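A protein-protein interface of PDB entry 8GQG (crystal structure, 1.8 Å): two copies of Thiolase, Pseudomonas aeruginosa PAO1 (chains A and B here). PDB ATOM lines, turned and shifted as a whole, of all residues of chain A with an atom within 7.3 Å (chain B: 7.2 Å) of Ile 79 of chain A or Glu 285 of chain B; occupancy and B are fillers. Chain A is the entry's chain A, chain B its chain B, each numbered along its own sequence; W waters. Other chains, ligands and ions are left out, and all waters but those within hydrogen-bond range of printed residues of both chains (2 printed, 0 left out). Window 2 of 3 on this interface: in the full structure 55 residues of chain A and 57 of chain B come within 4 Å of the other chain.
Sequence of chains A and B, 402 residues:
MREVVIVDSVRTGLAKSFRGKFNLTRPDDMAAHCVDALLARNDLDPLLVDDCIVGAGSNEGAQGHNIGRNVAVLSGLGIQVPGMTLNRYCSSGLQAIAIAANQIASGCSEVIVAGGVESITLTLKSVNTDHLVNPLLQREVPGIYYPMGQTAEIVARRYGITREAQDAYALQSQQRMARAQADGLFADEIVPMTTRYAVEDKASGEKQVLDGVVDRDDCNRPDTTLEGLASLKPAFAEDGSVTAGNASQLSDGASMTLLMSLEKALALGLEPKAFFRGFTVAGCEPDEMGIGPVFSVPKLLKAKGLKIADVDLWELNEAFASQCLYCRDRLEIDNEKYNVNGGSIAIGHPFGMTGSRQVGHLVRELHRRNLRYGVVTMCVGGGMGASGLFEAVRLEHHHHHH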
ATOM      1  N   LEU A  47      21.519 -10.488  19.522  1.00  0.00           N
ATOM      2  CA  LEU A  47      21.301 -10.864  18.103  1.00  0.00           C
ATOM      3  C   LEU A  47      21.000 -12.357  17.965  1.00  0.00           C
ATOM      4  O   LEU A  47      20.461 -12.723  16.936  1.00  0.00           O
ATOM      5  CB  LEU A  47      22.511 -10.408  17.263  1.00  0.00           C
ATOM      6  CG  LEU A  47      22.622  -8.879  17.117  1.00  0.00           C
ATOM      7  CD1 LEU A  47      23.496  -8.482  15.943  1.00  0.00           C
ATOM      8  CD2 LEU A  47      21.246  -8.222  16.972  1.00  0.00           C
ATOM      9  N   ARG A  69       6.475  -6.126  20.450  1.00  0.00           N
ATOM     10  CA  ARG A  69       7.501  -5.513  19.563  1.00  0.00           C
ATOM     11  C   ARG A  69       8.213  -4.355  20.292  1.00  0.00           C
ATOM     12  O   ARG A  69       9.449  -4.218  20.175  1.00  0.00           O
ATOM     13  CB  ARG A  69       6.906  -5.016  18.240  1.00  0.00           C
ATOM     14  CG  ARG A  69       7.843  -4.135  17.419  1.00  0.00           C
ATOM     15  CD  ARG A  69       9.129  -4.842  16.982  1.00  0.00           C
ATOM     16  NE  ARG A  69       9.829  -3.972  16.051  1.00  0.00           N
ATOM     17  CZ  ARG A  69      11.069  -4.131  15.596  1.00  0.00           C
ATOM     18  NH1 ARG A  69      11.553  -3.268  14.726  1.00  0.00           N
ATOM     19  NH2 ARG A  69      11.829  -5.117  16.024  1.00  0.00           N
ATOM     20  N   ALA A  72      10.759  -5.381  22.891  1.00  0.00           N
ATOM     21  CA  ALA A  72      12.003  -5.797  22.209  1.00  0.00           C
ATOM     22  C   ALA A  72      12.851  -4.539  21.873  1.00  0.00           C
ATOM     23  O   ALA A  72      14.065  -4.538  22.155  1.00  0.00           O
ATOM     24  CB  ALA A  72      11.660  -6.606  20.999  1.00  0.00           C
ATOM     25  N   VAL A  73      12.251  -3.529  21.252  1.00  0.00           N
ATOM     26  CA  VAL A  73      12.959  -2.309  20.762  1.00  0.00           C
ATOM     27  C   VAL A  73      13.494  -1.506  21.955  1.00  0.00           C
ATOM     28  O   VAL A  73      14.621  -1.042  21.889  1.00  0.00           O
ATOM     29  CB  VAL A  73      12.056  -1.483  19.835  1.00  0.00           C
ATOM     30  CG1 VAL A  73      12.768  -0.213  19.388  1.00  0.00           C
ATOM     31  CG2 VAL A  73      11.609  -2.290  18.625  1.00  0.00           C
ATOM     32  N   LEU A  74      12.734  -1.407  23.034  1.00  0.00           N
ATOM     33  CA  LEU A  74      13.134  -0.715  24.278  1.00  0.00           C
ATOM     34  C   LEU A  74      14.310  -1.438  24.926  1.00  0.00           C
ATOM     35  O   LEU A  74      15.179  -0.752  25.427  1.00  0.00           O
ATOM     36  CB  LEU A  74      11.975  -0.715  25.279  1.00  0.00           C
ATOM     37  CG  LEU A  74      10.961   0.397  25.090  1.00  0.00           C
ATOM     38  CD1 LEU A  74       9.686   0.095  25.890  1.00  0.00           C
ATOM     39  CD2 LEU A  74      11.551   1.736  25.491  1.00  0.00           C
ATOM     40  N   SER A  75      14.237  -2.762  25.011  1.00  0.00           N
ATOM     41  CA  SER A  75      15.296  -3.615  25.602  1.00  0.00           C
ATOM     42  C   SER A  75      16.593  -3.540  24.771  1.00  0.00           C
ATOM     43  O   SER A  75      16.621  -2.914  23.679  1.00  0.00           O
ATOM     44  CB  SER A  75      14.851  -5.060  25.730  1.00  0.00           C
ATOM     45  OG  SER A  75      14.927  -5.746  24.472  1.00  0.00           O
ATOM     46  N   GLY A  76      17.630  -4.210  25.276  1.00  0.00           N
ATOM     47  CA  GLY A  76      18.909  -4.411  24.577  1.00  0.00           C
ATOM     48  C   GLY A  76      18.721  -5.231  23.303  1.00  0.00           C
ATOM     49  O   GLY A  76      19.656  -5.248  22.507  1.00  0.00           O
ATOM     50  N   LEU A  77      17.563  -5.866  23.084  1.00  0.00           N
ATOM     51  CA  LEU A  77      17.283  -6.572  21.802  1.00  0.00           C
ATOM     52  C   LEU A  77      17.294  -5.578  20.644  1.00  0.00           C
ATOM     53  O   LEU A  77      17.900  -5.883  19.599  1.00  0.00           O
ATOM     54  CB  LEU A  77      15.958  -7.320  21.852  1.00  0.00           C
ATOM     55  CG  LEU A  77      15.815  -8.346  22.970  1.00  0.00           C
ATOM     56  CD1 LEU A  77      14.413  -8.917  23.020  1.00  0.00           C
ATOM     57  CD2 LEU A  77      16.845  -9.466  22.804  1.00  0.00           C
ATOM     58  N   GLY A  78      16.587  -4.453  20.772  1.00  0.00           N
ATOM     59  CA  GLY A  78      16.564  -3.425  19.709  1.00  0.00           C
ATOM     60  C   GLY A  78      15.756  -3.856  18.484  1.00  0.00           C
ATOM     61  O   GLY A  78      15.042  -4.886  18.537  1.00  0.00           O
ATOM     62  N   ILE A  79      15.861  -3.105  17.387  1.00  0.00           N
ATOM     63  CA  ILE A  79      14.976  -3.239  16.210  1.00  0.00           C
ATOM     64  C   ILE A  79      15.194  -4.583  15.522  1.00  0.00           C
ATOM     65  O   ILE A  79      14.275  -5.023  14.813  1.00  0.00           O
ATOM     66  CB  ILE A  79      15.155  -2.054  15.227  1.00  0.00           C
ATOM     67  CG1 ILE A  79      16.595  -1.931  14.711  1.00  0.00           C
ATOM     68  CG2 ILE A  79      14.693  -0.760  15.872  1.00  0.00           C
ATOM     69  CD1 ILE A  79      16.865  -2.691  13.440  1.00  0.00           C
ATOM     70  N   GLN A  80      16.339  -5.249  15.716  1.00  0.00           N
ATOM     71  CA  GLN A  80      16.621  -6.492  14.963  1.00  0.00           C
ATOM     72  C   GLN A  80      15.698  -7.613  15.426  1.00  0.00           C
ATOM     73  O   GLN A  80      15.528  -8.558  14.684  1.00  0.00           O
ATOM     74  CB  GLN A  80      18.059  -6.929  15.207  1.00  0.00           C
ATOM     75  CG  GLN A  80      19.036  -5.832  14.817  1.00  0.00           C
ATOM     76  CD  GLN A  80      19.685  -6.201  13.517  1.00  0.00           C
ATOM     77  OE1 GLN A  80      20.776  -6.773  13.511  1.00  0.00           O
ATOM     78  NE2 GLN A  80      18.980  -5.920  12.427  1.00  0.00           N
ATOM     79  N   VAL A  81      15.158  -7.523  16.633  1.00  0.00           N
ATOM     80  CA  VAL A  81      14.348  -8.631  17.202  1.00  0.00           C
ATOM     81  C   VAL A  81      12.862  -8.280  17.100  1.00  0.00           C
ATOM     82  O   VAL A  81      12.391  -7.331  17.708  1.00  0.00           O
ATOM     83  CB  VAL A  81      14.783  -8.951  18.647  1.00  0.00           C
ATOM     84  CG1 VAL A  81      13.973 -10.114  19.190  1.00  0.00           C
ATOM     85  CG2 VAL A  81      16.291  -9.233  18.717  1.00  0.00           C
ATOM     86  N   PRO A  82      12.070  -9.130  16.432  1.00  0.00           N
ATOM     87  CA  PRO A  82      10.617  -8.933  16.312  1.00  0.00           C
ATOM     88  C   PRO A  82       9.921  -9.214  17.655  1.00  0.00           C
ATOM     89  O   PRO A  82      10.531  -9.860  18.586  1.00  0.00           O
ATOM     90  CB  PRO A  82      10.247  -9.928  15.205  1.00  0.00           C
ATOM     91  CG  PRO A  82      11.259 -11.038  15.317  1.00  0.00           C
ATOM     92  CD  PRO A  82      12.527 -10.358  15.789  1.00  0.00           C
ATOM     93  N   GLU B 140      14.197   7.394  21.033  1.00  0.00           N
ATOM     94  CA  GLU B 140      15.228   6.408  20.596  1.00  0.00           C
ATOM     95  C   GLU B 140      14.914   5.922  19.169  1.00  0.00           C
ATOM     96  O   GLU B 140      15.833   5.857  18.356  1.00  0.00           O
ATOM     97  CB  GLU B 140      15.292   5.216  21.561  1.00  0.00           C
ATOM     98  CG  GLU B 140      15.834   5.535  22.952  1.00  0.00           C
ATOM     99  CD  GLU B 140      15.866   4.374  23.953  1.00  0.00           C
ATOM    100  OE1 GLU B 140      15.277   3.290  23.684  1.00  0.00           O
ATOM    101  OE2 GLU B 140      16.476   4.543  25.012  1.00  0.00           O
ATOM    102  N   VAL B 141      13.655   5.566  18.872  1.00  0.00           N
ATOM    103  CA  VAL B 141      13.259   4.958  17.574  1.00  0.00           C
ATOM    104  C   VAL B 141      11.949   5.601  17.131  1.00  0.00           C
ATOM    105  O   VAL B 141      10.889   4.991  17.189  1.00  0.00           O
ATOM    106  CB  VAL B 141      13.160   3.418  17.681  1.00  0.00           C
ATOM    107  CG1 VAL B 141      13.051   2.806  16.295  1.00  0.00           C
ATOM    108  CG2 VAL B 141      14.349   2.818  18.423  1.00  0.00           C
ATOM    109  N   GLY B 143      10.633   6.071  14.380  1.00  0.00           N
ATOM    110  CA  GLY B 143      10.044   5.239  13.325  1.00  0.00           C
ATOM    111  C   GLY B 143       8.918   4.352  13.833  1.00  0.00           C
ATOM    112  O   GLY B 143       8.025   4.036  13.019  1.00  0.00           O
ATOM    113  N   ILE B 144       8.957   3.959  15.101  1.00  0.00           N
ATOM    114  CA  ILE B 144       7.911   3.086  15.730  1.00  0.00           C
ATOM    115  C   ILE B 144       6.530   3.745  15.568  1.00  0.00           C
ATOM    116  O   ILE B 144       5.502   3.029  15.579  1.00  0.00           O
ATOM    117  CB  ILE B 144       8.253   2.781  17.208  1.00  0.00           C
ATOM    118  CG1 ILE B 144       9.333   1.705  17.324  1.00  0.00           C
ATOM    119  CG2 ILE B 144       7.028   2.356  18.016  1.00  0.00           C
ATOM    120  CD1 ILE B 144       8.824   0.296  17.071  1.00  0.00           C
ATOM    121  N   THR B 151       6.414   5.281   5.845  1.00  0.00           N
ATOM    122  CA  THR B 151       7.491   4.281   5.701  1.00  0.00           C
ATOM    123  C   THR B 151       7.500   3.843   4.232  1.00  0.00           C
ATOM    124  O   THR B 151       8.591   3.549   3.711  1.00  0.00           O
ATOM    125  CB  THR B 151       7.334   3.111   6.689  1.00  0.00           C
ATOM    126  OG1 THR B 151       6.298   2.271   6.209  1.00  0.00           O
ATOM    127  CG2 THR B 151       6.992   3.525   8.101  1.00  0.00           C
ATOM    128  N   ARG B 158      14.642   5.561  -0.450  1.00  0.00           N
ATOM    129  CA  ARG B 158      15.906   4.928   0.023  1.00  0.00           C
ATOM    130  C   ARG B 158      16.386   3.901  -0.995  1.00  0.00           C
ATOM    131  O   ARG B 158      17.581   3.834  -1.212  1.00  0.00           O
ATOM    132  CB  ARG B 158      15.683   4.286   1.394  1.00  0.00           C
ATOM    133  CG  ARG B 158      16.947   3.778   2.055  1.00  0.00           C
ATOM    134  CD  ARG B 158      16.632   3.417   3.489  1.00  0.00           C
ATOM    135  NE  ARG B 158      16.381   4.577   4.335  1.00  0.00           N
ATOM    136  CZ  ARG B 158      15.766   4.520   5.514  1.00  0.00           C
ATOM    137  NH1 ARG B 158      15.609   5.620   6.217  1.00  0.00           N
ATOM    138  NH2 ARG B 158      15.281   3.377   5.985  1.00  0.00           N
ATOM    139  N   ALA B 282      11.396 -11.683  11.581  1.00  0.00           N
ATOM    140  CA  ALA B 282      12.671 -10.960  11.661  1.00  0.00           C
ATOM    141  C   ALA B 282      12.311  -9.513  11.939  1.00  0.00           C
ATOM    142  O   ALA B 282      11.197  -9.105  11.560  1.00  0.00           O
ATOM    143  CB  ALA B 282      13.459 -11.102  10.375  1.00  0.00           C
ATOM    144  N   GLY B 283      13.236  -8.787  12.548  1.00  0.00           N
ATOM    145  CA  GLY B 283      13.073  -7.380  12.878  1.00  0.00           C
ATOM    146  C   GLY B 283      13.787  -6.545  11.837  1.00  0.00           C
ATOM    147  O   GLY B 283      14.761  -7.054  11.221  1.00  0.00           O
ATOM    148  N   CYS B 284      13.336  -5.321  11.627  1.00  0.00           N
ATOM    149  CA  CYS B 284      14.075  -4.357  10.802  1.00  0.00           C
ATOM    150  C   CYS B 284      13.769  -2.962  11.328  1.00  0.00           C
ATOM    151  O   CYS B 284      13.001  -2.846  12.282  1.00  0.00           O
ATOM    152  CB  CYS B 284      13.769  -4.582   9.328  1.00  0.00           C
ATOM    153  SG  CYS B 284      12.077  -4.150   8.859  1.00  0.00           S
ATOM    154  N   GLU B 285      14.332  -1.938  10.693  1.00  0.00           N
ATOM    155  CA  GLU B 285      14.088  -0.538  11.095  1.00  0.00           C
ATOM    156  C   GLU B 285      12.609  -0.236  10.878  1.00  0.00           C
ATOM    157  O   GLU B 285      12.054  -0.531   9.808  1.00  0.00           O
ATOM    158  CB  GLU B 285      14.998   0.399  10.300  1.00  0.00           C
ATOM    159  CG  GLU B 285      16.420   0.421  10.824  1.00  0.00           C
ATOM    160  CD  GLU B 285      16.581   1.111  12.158  1.00  0.00           C
ATOM    161  OE1 GLU B 285      17.664   0.966  12.720  1.00  0.00           O
ATOM    162  OE2 GLU B 285      15.604   1.735  12.656  1.00  0.00           O
ATOM    163  N   PRO B 286      11.886   0.308  11.869  1.00  0.00           N
ATOM    164  CA  PRO B 286      10.464   0.623  11.671  1.00  0.00           C
ATOM    165  C   PRO B 286      10.201   1.571  10.487  1.00  0.00           C
ATOM    166  O   PRO B 286       9.150   1.447   9.834  1.00  0.00           O
ATOM    167  CB  PRO B 286      10.031   1.320  12.976  1.00  0.00           C
ATOM    168  CG  PRO B 286      11.074   0.962  13.998  1.00  0.00           C
ATOM    169  CD  PRO B 286      12.316   0.490  13.256  1.00  0.00           C
ATOM    170  N   ASP B 287      11.135   2.506  10.244  1.00  0.00           N
ATOM    171  CA  ASP B 287      10.934   3.545   9.212  1.00  0.00           C
ATOM    172  C   ASP B 287      10.940   2.900   7.838  1.00  0.00           C
ATOM    173  O   ASP B 287      10.506   3.574   6.892  1.00  0.00           O
ATOM    174  CB  ASP B 287      11.919   4.715   9.343  1.00  0.00           C
ATOM    175  CG  ASP B 287      13.341   4.482   8.883  1.00  0.00           C
ATOM    176  OD1 ASP B 287      13.715   3.343   8.504  1.00  0.00           O
ATOM    177  OD2 ASP B 287      14.064   5.483   8.879  1.00  0.00           O
ATOM    178  N   GLU B 288      11.439   1.665   7.710  1.00  0.00           N
ATOM    179  CA  GLU B 288      11.400   0.945   6.420  1.00  0.00           C
ATOM    180  C   GLU B 288      10.760  -0.431   6.641  1.00  0.00           C
ATOM    181  O   GLU B 288      11.187  -1.415   6.052  1.00  0.00           O
ATOM    182  CB  GLU B 288      12.796   0.905   5.789  1.00  0.00           C
ATOM    183  CG  GLU B 288      13.878   0.337   6.696  1.00  0.00           C
ATOM    184  CD  GLU B 288      15.292   0.270   6.097  1.00  0.00           C
ATOM    185  OE1 GLU B 288      15.511   0.836   4.999  1.00  0.00           O
ATOM    186  OE2 GLU B 288      16.171  -0.365   6.733  1.00  0.00           O
ATOM    187  N   MET B 289       9.685  -0.478   7.409  1.00  0.00           N
ATOM    188  CA  MET B 289       9.040  -1.764   7.767  1.00  0.00           C
ATOM    189  C   MET B 289       8.685  -2.555   6.502  1.00  0.00           C
ATOM    190  O   MET B 289       8.745  -3.808   6.562  1.00  0.00           O
ATOM    191  CB  MET B 289       7.799  -1.516   8.623  1.00  0.00           C
ATOM    192  CG  MET B 289       6.669  -0.838   7.865  1.00  0.00           C
ATOM    193  SD  MET B 289       5.533  -2.033   7.204  1.00  0.00           S
ATOM    194  CE  MET B 289       4.738  -1.116   5.877  1.00  0.00           C
ATOM    195  N   GLY B 290       8.425  -1.894   5.365  1.00  0.00           N
ATOM    196  CA  GLY B 290       8.054  -2.595   4.129  1.00  0.00           C
ATOM    197  C   GLY B 290       9.072  -3.670   3.695  1.00  0.00           C
ATOM    198  O   GLY B 290       8.696  -4.564   2.947  1.00  0.00           O
ATOM    199  N   ILE B 291      10.341  -3.539   4.064  1.00  0.00           N
ATOM    200  CA  ILE B 291      11.393  -4.480   3.570  1.00  0.00           C
ATOM    201  C   ILE B 291      11.454  -5.715   4.475  1.00  0.00           C
ATOM    202  O   ILE B 291      12.206  -6.643   4.140  1.00  0.00           O
ATOM    203  CB  ILE B 291      12.748  -3.767   3.443  1.00  0.00           C
ATOM    204  CG1 ILE B 291      13.468  -3.531   4.772  1.00  0.00           C
ATOM    205  CG2 ILE B 291      12.559  -2.467   2.692  1.00  0.00           C
ATOM    206  CD1 ILE B 291      14.951  -3.209   4.595  1.00  0.00           C
ATOM    207  N   GLY B 292      10.679  -5.757   5.565  1.00  0.00           N
ATOM    208  CA  GLY B 292      10.635  -6.943   6.461  1.00  0.00           C
ATOM    209  C   GLY B 292      10.942  -8.300   5.805  1.00  0.00           C
ATOM    210  O   GLY B 292      11.823  -9.040   6.291  1.00  0.00           O
ATOM    211  N   PHE B 295      14.391 -10.069   5.281  1.00  0.00           N
ATOM    212  CA  PHE B 295      15.098 -10.630   6.467  1.00  0.00           C
ATOM    213  C   PHE B 295      14.435 -11.946   6.917  1.00  0.00           C
ATOM    214  O   PHE B 295      15.149 -12.914   7.339  1.00  0.00           O
ATOM    215  CB  PHE B 295      15.161  -9.593   7.594  1.00  0.00           C
ATOM    216  CG  PHE B 295      15.899  -8.339   7.204  1.00  0.00           C
ATOM    217  CD1 PHE B 295      17.288  -8.344   7.078  1.00  0.00           C
ATOM    218  CD2 PHE B 295      15.214  -7.169   6.903  1.00  0.00           C
ATOM    219  CE1 PHE B 295      17.977  -7.198   6.680  1.00  0.00           C
ATOM    220  CE2 PHE B 295      15.903  -6.029   6.513  1.00  0.00           C
ATOM    221  CZ  PHE B 295      17.282  -6.040   6.397  1.00  0.00           C
ATOM    222  N   VAL B 380       5.378  -5.892   8.207  1.00  0.00           N
ATOM    223  CA  VAL B 380       4.554  -5.671   9.412  1.00  0.00           C
ATOM    224  C   VAL B 380       4.920  -4.304   9.969  1.00  0.00           C
ATOM    225  O   VAL B 380       6.115  -4.050  10.244  1.00  0.00           O
ATOM    226  CB  VAL B 380       4.812  -6.753  10.469  1.00  0.00           C
ATOM    227  CG1 VAL B 380       3.891  -6.569  11.656  1.00  0.00           C
ATOM    228  CG2 VAL B 380       4.667  -8.140   9.868  1.00  0.00           C
ATOM    229  N   GLY B 382       5.755  -1.511  12.453  1.00  0.00           N
ATOM    230  CA  GLY B 382       6.673  -1.637  13.610  1.00  0.00           C
ATOM    231  C   GLY B 382       8.055  -2.176  13.224  1.00  0.00           C
ATOM    232  O   GLY B 382       8.975  -2.119  14.059  1.00  0.00           O
ATOM    233  N   GLY B 383       8.200  -2.684  12.007  1.00  0.00           N
ATOM    234  CA  GLY B 383       9.476  -3.124  11.419  1.00  0.00           C
ATOM    235  C   GLY B 383       9.687  -4.608  11.643  1.00  0.00           C
ATOM    236  O   GLY B 383      10.596  -4.956  12.384  1.00  0.00           O
ATOM    237  N   MET B 384       8.863  -5.445  11.017  1.00  0.00           N
ATOM    238  CA  MET B 384       9.090  -6.897  10.958  1.00  0.00           C
ATOM    239  C   MET B 384       8.736  -7.449   9.574  1.00  0.00           C
ATOM    240  O   MET B 384       8.019  -6.808   8.770  1.00  0.00           O
ATOM    241  CB  MET B 384       8.281  -7.635  12.040  1.00  0.00           C
ATOM    242  CG  MET B 384       8.623  -7.190  13.441  1.00  0.00           C
ATOM    243  SD  MET B 384       7.510  -7.857  14.655  1.00  0.00           S
ATOM    244  CE  MET B 384       6.176  -6.642  14.654  1.00  0.00           C
HETATM  245  O   HOH W   1      15.526   1.856  26.784  1.00  0.00           O
HETATM  246  O   HOH W   2      15.597 -10.783  13.128  1.00  0.00           O
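CG1 of Val 73 of chain A touches CG2 of Val 141 of chain B, at 3.6 Å.
CG1 of Val 141 of chain B touches CG2 of Ile 79 of chain A, at 3.9 Å.
Gly 283 of chain B touches Ile 79 of chain A (CA to O, 3.3 Å).
CG1 of Ile 79 of chain A touches OE1 of Glu 285 of chain B, at 3.7 Å.
Ile 79 of chain A touches Pro 286 of chain B (CG2 to CD, 3.7 Å).
Ala 282 of chain B touches Pro 82 of chain A.
Pro 82 of chain A touches Gly 283 of chain B.
Met 384 of chain B touches Pro 82 of chain A.
Of the 22 printed residues of chain B, 9 touch a printed residue of chain A.
Hydrophobic or aromatic side chains of chain B within 4 Å of the printed part of chain A: Val 141, Pro 286 and Met 384.
Along chain B the printed residues that touch a printed residue of chain A span positions 141 to 384.
Among the printed residues, 13 pairs touch across the chains.
NH2 of Arg 69 of chain A sits at hydrogen-bond distance from O of Ile 79 of chain A (2.7 Å).
NH2 of Arg 69 of chain A is in hydrogen-bond range of O of Val 81 of chain A (2.8 Å).
The backbone NH of Cys 284 of chain B lies within hydrogen-bond range of the backbone carbonyl oxygen of Gly 383 of chain B (2.9 Å).
The backbone NH (N) of Gly 283 of chain B is in hydrogen-bond range of the backbone carbonyl oxygen (O) of Gln 80 of chain A.
The backbone carbonyl oxygen (O) of Ile 79 of chain A is in hydrogen-bond range of the backbone NH (N) of Cys 284 of chain B.
NH1 of Arg 69 of chain A sits at hydrogen-bond distance from O of Gly 383 of chain B, at 3.0 Å.
O of Gly 382 of chain B sits at hydrogen-bond distance from NE of Arg 69 of chain A (2.9 Å).
The guanidinium group of Arg 69 of chain A sits at hydrogen-bond distance from the backbone carbonyl oxygen of Cys 284 of chain B, 2.9 Å away.
Water W2 lies within hydrogen-bond range of O of Gln 80 of chain A (2.7 Å) and N of Gly 283 of chain B (3.1 Å).
Water W1 lies within hydrogen-bond range of O of Leu 74 of chain A and OE2 of Glu 140 of chain B.
Printed residues of chain B within 4 Å of Ile 79 of chain A: Val 141, Gly 283, Cys 284, Glu 285 and Pro 286.
Glu 285 of chain B touches one residue of chain A.
Printed residues of chain A within 4 Å of Cys 284 of chain B: Arg 69 (2.9 Å) and Ile 79 (3.3 Å).
Of the printed residues of chain A, Gly 382 of chain B touches Arg 69.
Of the printed residues of chain A, Val 141 of chain B touches Val 73 (3.6 Å) and Ile 79 (3.9 Å).
Of the printed residues of chain A, Pro 286 of chain B touches Ile 79.
Thr 151 of chain B touches none of the printed residues of chain A.
The nearest residue of chain B that does not touch Ile 79 of chain A is Gly 383 of chain B (4.4 Å).
The nearest printed residue of chain B that does not touch Arg 69 of chain A is Met 384 of chain B (4.005 Å).
No position is printed for both chains.
Of the 13 pairs that touch across the chains among the printed residues, none has its exchanged pair printed and touching as well.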
